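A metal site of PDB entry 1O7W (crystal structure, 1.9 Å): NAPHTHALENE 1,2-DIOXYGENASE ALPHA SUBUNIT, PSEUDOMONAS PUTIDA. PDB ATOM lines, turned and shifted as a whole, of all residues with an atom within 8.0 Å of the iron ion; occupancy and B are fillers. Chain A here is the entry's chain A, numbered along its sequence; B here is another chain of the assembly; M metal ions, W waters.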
ATOM      1  N   ASN A 201      38.023   3.233  21.055  1.00  0.00           N
ATOM      2  CA  ASN A 201      36.920   2.994  20.152  1.00  0.00           C
ATOM      3  C   ASN A 201      37.186   3.721  18.831  1.00  0.00           C
ATOM      4  O   ASN A 201      37.105   3.115  17.747  1.00  0.00           O
ATOM      5  CB  ASN A 201      35.605   3.402  20.820  1.00  0.00           C
ATOM      6  CG  ASN A 201      34.408   3.259  19.883  1.00  0.00           C
ATOM      7  OD1 ASN A 201      33.981   4.229  19.259  1.00  0.00           O
ATOM      8  ND2 ASN A 201      33.850   2.055  19.787  1.00  0.00           N
ATOM      9  N   PHE A 202      37.556   5.003  18.912  1.00  0.00           N
ATOM     10  CA  PHE A 202      37.912   5.759  17.705  1.00  0.00           C
ATOM     11  C   PHE A 202      39.237   5.353  17.049  1.00  0.00           C
ATOM     12  O   PHE A 202      39.381   5.507  15.835  1.00  0.00           O
ATOM     13  CB  PHE A 202      37.961   7.270  17.974  1.00  0.00           C
ATOM     14  CG  PHE A 202      36.633   7.943  17.903  1.00  0.00           C
ATOM     15  CD1 PHE A 202      35.621   7.606  18.783  1.00  0.00           C
ATOM     16  CD2 PHE A 202      36.395   8.930  16.955  1.00  0.00           C
ATOM     17  CE1 PHE A 202      34.370   8.226  18.714  1.00  0.00           C
ATOM     18  CE2 PHE A 202      35.149   9.557  16.880  1.00  0.00           C
ATOM     19  CZ  PHE A 202      34.141   9.203  17.761  1.00  0.00           C
ATOM     20  N   ASP A 205      38.213   0.759  16.181  1.00  0.00           N
ATOM     21  CA  ASP A 205      37.035  -0.079  16.290  1.00  0.00           C
ATOM     22  C   ASP A 205      36.057   0.022  15.119  1.00  0.00           C
ATOM     23  O   ASP A 205      35.032   0.676  15.218  1.00  0.00           O
ATOM     24  CB  ASP A 205      36.299   0.213  17.596  1.00  0.00           C
ATOM     25  CG  ASP A 205      35.377  -0.901  17.987  1.00  0.00           C
ATOM     26  OD1 ASP A 205      35.096  -1.025  19.208  1.00  0.00           O
ATOM     27  OD2 ASP A 205      34.896  -1.719  17.145  1.00  0.00           O
ATOM     28  N   HIS A 208      32.565  -2.672  15.751  1.00  0.00           N
ATOM     29  CA  HIS A 208      31.325  -2.353  16.484  1.00  0.00           C
ATOM     30  C   HIS A 208      30.273  -1.629  15.643  1.00  0.00           C
ATOM     31  O   HIS A 208      29.099  -1.634  15.992  1.00  0.00           O
ATOM     32  CB  HIS A 208      31.622  -1.524  17.743  1.00  0.00           C
ATOM     33  CG  HIS A 208      31.689  -0.049  17.507  1.00  0.00           C
ATOM     34  ND1 HIS A 208      32.685   0.541  16.748  1.00  0.00           N
ATOM     35  CD2 HIS A 208      30.877   0.959  17.906  1.00  0.00           C
ATOM     36  CE1 HIS A 208      32.479   1.849  16.703  1.00  0.00           C
ATOM     37  NE2 HIS A 208      31.390   2.123  17.402  1.00  0.00           N
ATOM     38  N   VAL A 209      30.698  -1.027  14.540  1.00  0.00           N
ATOM     39  CA  VAL A 209      29.830  -0.102  13.802  1.00  0.00           C
ATOM     40  C   VAL A 209      28.507  -0.728  13.373  1.00  0.00           C
ATOM     41  O   VAL A 209      27.446  -0.161  13.641  1.00  0.00           O
ATOM     42  CB  VAL A 209      30.545   0.572  12.607  1.00  0.00           C
ATOM     43  CG1 VAL A 209      29.564   1.472  11.792  1.00  0.00           C
ATOM     44  CG2 VAL A 209      31.747   1.387  13.111  1.00  0.00           C
ATOM     45  N   GLY A 210      28.560  -1.894  12.731  1.00  0.00           N
ATOM     46  CA  GLY A 210      27.356  -2.555  12.235  1.00  0.00           C
ATOM     47  C   GLY A 210      26.341  -2.948  13.298  1.00  0.00           C
ATOM     48  O   GLY A 210      25.117  -2.905  13.042  1.00  0.00           O
ATOM     49  N   THR A 212      26.551  -1.887  17.051  1.00  0.00           N
ATOM     50  CA  THR A 212      26.268  -0.754  17.943  1.00  0.00           C
ATOM     51  C   THR A 212      25.392   0.283  17.282  1.00  0.00           C
ATOM     52  O   THR A 212      24.430   0.784  17.865  1.00  0.00           O
ATOM     53  CB  THR A 212      27.568  -0.062  18.397  1.00  0.00           C
ATOM     54  OG1 THR A 212      28.218  -0.851  19.406  1.00  0.00           O
ATOM     55  CG2 THR A 212      27.276   1.261  19.116  1.00  0.00           C
ATOM     56  N   HIS A 213      25.750   0.613  16.038  1.00  0.00           N
ATOM     57  CA  HIS A 213      25.087   1.690  15.302  1.00  0.00           C
ATOM     58  C   HIS A 213      24.067   1.206  14.295  1.00  0.00           C
ATOM     59  O   HIS A 213      23.692   1.957  13.408  1.00  0.00           O
ATOM     60  CB  HIS A 213      26.124   2.579  14.587  1.00  0.00           C
ATOM     61  CG  HIS A 213      27.073   3.265  15.528  1.00  0.00           C
ATOM     62  ND1 HIS A 213      26.667   4.258  16.393  1.00  0.00           N
ATOM     63  CD2 HIS A 213      28.404   3.097  15.739  1.00  0.00           C
ATOM     64  CE1 HIS A 213      27.702   4.668  17.102  1.00  0.00           C
ATOM     65  NE2 HIS A 213      28.767   3.981  16.724  1.00  0.00           N
ATOM     66  N   LEU A 307      37.171  11.728  12.882  1.00  0.00           N
ATOM     67  CA  LEU A 307      36.695  10.998  11.717  1.00  0.00           C
ATOM     68  C   LEU A 307      36.861  11.980  10.570  1.00  0.00           C
ATOM     69  O   LEU A 307      36.106  12.949  10.477  1.00  0.00           O
ATOM     70  CB  LEU A 307      35.217  10.615  11.839  1.00  0.00           C
ATOM     71  CG  LEU A 307      34.762   9.857  13.102  1.00  0.00           C
ATOM     72  CD1 LEU A 307      33.292   9.537  13.035  1.00  0.00           C
ATOM     73  CD2 LEU A 307      35.583   8.586  13.350  1.00  0.00           C
ATOM     74  N   PHE A 352      27.214  13.248  15.942  1.00  0.00           N
ATOM     75  CA  PHE A 352      28.194  12.992  16.993  1.00  0.00           C
ATOM     76  C   PHE A 352      28.295  14.029  18.122  1.00  0.00           C
ATOM     77  O   PHE A 352      29.157  13.921  18.999  1.00  0.00           O
ATOM     78  CB  PHE A 352      29.575  12.729  16.363  1.00  0.00           C
ATOM     79  CG  PHE A 352      29.736  11.307  15.916  1.00  0.00           C
ATOM     80  CD1 PHE A 352      30.221  10.343  16.799  1.00  0.00           C
ATOM     81  CD2 PHE A 352      29.339  10.911  14.654  1.00  0.00           C
ATOM     82  CE1 PHE A 352      30.333   9.012  16.423  1.00  0.00           C
ATOM     83  CE2 PHE A 352      29.465   9.595  14.253  1.00  0.00           C
ATOM     84  CZ  PHE A 352      29.946   8.642  15.128  1.00  0.00           C
ATOM     85  N   TRP A 358      24.241   9.049  16.610  1.00  0.00           N
ATOM     86  CA  TRP A 358      25.279   8.008  16.570  1.00  0.00           C
ATOM     87  C   TRP A 358      26.024   7.901  17.893  1.00  0.00           C
ATOM     88  O   TRP A 358      26.190   6.802  18.437  1.00  0.00           O
ATOM     89  CB  TRP A 358      26.332   8.268  15.483  1.00  0.00           C
ATOM     90  CG  TRP A 358      25.808   8.126  14.079  1.00  0.00           C
ATOM     91  CD1 TRP A 358      24.852   8.893  13.467  1.00  0.00           C
ATOM     92  CD2 TRP A 358      26.248   7.179  13.102  1.00  0.00           C
ATOM     93  NE1 TRP A 358      24.668   8.466  12.171  1.00  0.00           N
ATOM     94  CE2 TRP A 358      25.510   7.426  11.923  1.00  0.00           C
ATOM     95  CE3 TRP A 358      27.202   6.157  13.102  1.00  0.00           C
ATOM     96  CZ2 TRP A 358      25.682   6.666  10.759  1.00  0.00           C
ATOM     97  CZ3 TRP A 358      27.379   5.415  11.949  1.00  0.00           C
ATOM     98  CH2 TRP A 358      26.623   5.665  10.794  1.00  0.00           C
ATOM     99  N   GLU A 359      26.494   9.042  18.397  1.00  0.00           N
ATOM    100  CA  GLU A 359      27.283   9.102  19.640  1.00  0.00           C
ATOM    101  C   GLU A 359      26.503   8.472  20.815  1.00  0.00           C
ATOM    102  O   GLU A 359      27.091   7.784  21.658  1.00  0.00           O
ATOM    103  CB  GLU A 359      27.715  10.560  19.923  1.00  0.00           C
ATOM    104  CG  GLU A 359      28.535  10.811  21.194  1.00  0.00           C
ATOM    105  CD  GLU A 359      30.060  10.766  21.036  1.00  0.00           C
ATOM    106  OE1 GLU A 359      30.561  10.175  20.046  1.00  0.00           O
ATOM    107  OE2 GLU A 359      30.765  11.309  21.931  1.00  0.00           O
ATOM    108  N   SER A 360      25.183   8.677  20.842  1.00  0.00           N
ATOM    109  CA  SER A 360      24.338   8.090  21.885  1.00  0.00           C
ATOM    110  C   SER A 360      24.323   6.556  21.873  1.00  0.00           C
ATOM    111  O   SER A 360      24.229   5.931  22.944  1.00  0.00           O
ATOM    112  CB  SER A 360      22.900   8.627  21.785  1.00  0.00           C
ATOM    113  OG  SER A 360      22.195   7.980  20.741  1.00  0.00           O
ATOM    114  N   ASP A 361      24.457   5.952  20.690  1.00  0.00           N
ATOM    115  CA  ASP A 361      24.567   4.491  20.605  1.00  0.00           C
ATOM    116  C   ASP A 361      25.753   3.961  21.405  1.00  0.00           C
ATOM    117  O   ASP A 361      25.708   2.839  21.898  1.00  0.00           O
ATOM    118  CB  ASP A 361      24.784   4.013  19.158  1.00  0.00           C
ATOM    119  CG  ASP A 361      23.644   4.390  18.208  1.00  0.00           C
ATOM    120  OD1 ASP A 361      23.901   4.474  16.969  1.00  0.00           O
ATOM    121  OD2 ASP A 361      22.472   4.617  18.593  1.00  0.00           O
ATOM    122  N   ASP A 362      26.821   4.761  21.481  1.00  0.00           N
ATOM    123  CA  ASP A 362      28.072   4.336  22.121  1.00  0.00           C
ATOM    124  C   ASP A 362      28.096   4.526  23.619  1.00  0.00           C
ATOM    125  O   ASP A 362      28.978   3.986  24.286  1.00  0.00           O
ATOM    126  CB  ASP A 362      29.226   5.154  21.547  1.00  0.00           C
ATOM    127  CG  ASP A 362      29.619   4.709  20.169  1.00  0.00           C
ATOM    128  OD1 ASP A 362      29.707   5.579  19.288  1.00  0.00           O
ATOM    129  OD2 ASP A 362      29.867   3.516  19.883  1.00  0.00           O
ATOM    130  N   ASN A 363      27.152   5.313  24.156  1.00  0.00           N
ATOM    131  CA  ASN A 363      27.178   5.719  25.562  1.00  0.00           C
ATOM    132  C   ASN A 363      27.263   4.528  26.484  1.00  0.00           C
ATOM    133  O   ASN A 363      28.202   4.446  27.299  1.00  0.00           O
ATOM    134  CB  ASN A 363      25.939   6.517  25.962  1.00  0.00           C
ATOM    135  CG  ASN A 363      26.020   7.998  25.582  1.00  0.00           C
ATOM    136  OD1 ASN A 363      25.063   8.775  25.748  1.00  0.00           O
ATOM    137  ND2 ASN A 363      27.200   8.402  25.062  1.00  0.00           N
ATOM    138  N   ASN A 365      27.960   1.400  25.912  1.00  0.00           N
ATOM    139  CA  ASN A 365      29.164   0.616  25.680  1.00  0.00           C
ATOM    140  C   ASN A 365      30.325   1.156  26.499  1.00  0.00           C
ATOM    141  O   ASN A 365      30.996   0.418  27.225  1.00  0.00           O
ATOM    142  CB  ASN A 365      29.598   0.650  24.207  1.00  0.00           C
ATOM    143  CG  ASN A 365      28.601   0.007  23.259  1.00  0.00           C
ATOM    144  OD1 ASN A 365      27.775  -0.772  23.678  1.00  0.00           O
ATOM    145  ND2 ASN A 365      28.674   0.363  21.980  1.00  0.00           N
ATOM    146  N   MET A 366      30.584   2.444  26.363  1.00  0.00           N
ATOM    147  CA  MET A 366      31.718   3.064  27.020  1.00  0.00           C
ATOM    148  C   MET A 366      31.559   3.154  28.526  1.00  0.00           C
ATOM    149  O   MET A 366      32.513   2.910  29.277  1.00  0.00           O
ATOM    150  CB  MET A 366      31.917   4.492  26.550  1.00  0.00           C
ATOM    151  CG  MET A 366      31.576   4.690  25.129  1.00  0.00           C
ATOM    152  SD  MET A 366      33.059   4.970  24.264  1.00  0.00           S
ATOM    153  CE  MET A 366      33.561   3.393  24.141  1.00  0.00           C
ATOM    154  N   TYR B 103      27.740  -4.288  22.014  1.00  0.00           N
ATOM    155  CA  TYR B 103      28.930  -3.572  21.543  1.00  0.00           C
ATOM    156  C   TYR B 103      29.367  -4.132  20.152  1.00  0.00           C
ATOM    157  O   TYR B 103      29.250  -3.434  19.132  1.00  0.00           O
ATOM    158  CB  TYR B 103      30.028  -3.614  22.601  1.00  0.00           C
ATOM    159  CG  TYR B 103      31.105  -2.532  22.508  1.00  0.00           C
ATOM    160  CD1 TYR B 103      32.013  -2.320  23.552  1.00  0.00           C
ATOM    161  CD2 TYR B 103      31.208  -1.723  21.382  1.00  0.00           C
ATOM    162  CE1 TYR B 103      33.026  -1.364  23.445  1.00  0.00           C
ATOM    163  CE2 TYR B 103      32.204  -0.747  21.286  1.00  0.00           C
ATOM    164  CZ  TYR B 103      33.124  -0.568  22.317  1.00  0.00           C
ATOM    165  OH  TYR B 103      34.105   0.375  22.221  1.00  0.00           O
HETATM  166 FE    FE M   1      30.541   3.955  17.757  1.00  0.00          FE
HETATM  167  O   HOH W   1      32.127   5.556  17.371  1.00  0.00           O
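The iron ion is bound by a ring nitrogen (NE2) of His 208 (2.1 Å), a ring nitrogen (NE2) of His 213 (2.1 Å), the side-chain carboxylate (OD2) of Asp 362 (2.3 Å), water W1 (2.3 Å) and the side-chain carboxylate (OD1) of Asp 362 (2.4 Å).
A ring nitrogen (ND1) of His 208 sits at hydrogen-bond distance from the backbone carbonyl oxygen (O) of Asp 205 (2.8 Å). The side-chain amide nitrogen (ND2) of Asn 201 sits at hydrogen-bond distance from the side-chain hydroxyl (OH) of Tyr 103 of chain B (3.0 Å). ND2 of Asn 201 sits close to NE2 of His 208 (3.4 Å). The side-chain amide nitrogen (ND2) of Asn 201 sits at hydrogen-bond distance from the side-chain carboxylate (OD1) of Asp 205 (3.4 Å). ND1 of His 213 is in hydrogen-bond range of OD1 of Asp 361 (2.8 Å). A ring nitrogen (ND1) of His 213 lies close to the backbone carbonyl oxygen of Trp 358, at 3.3 Å.
Merely in contact with the iron ion: Asn 201 (3.8 Å). Of the 19 residues printed, 4 come within 4 Å of the iron ion.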
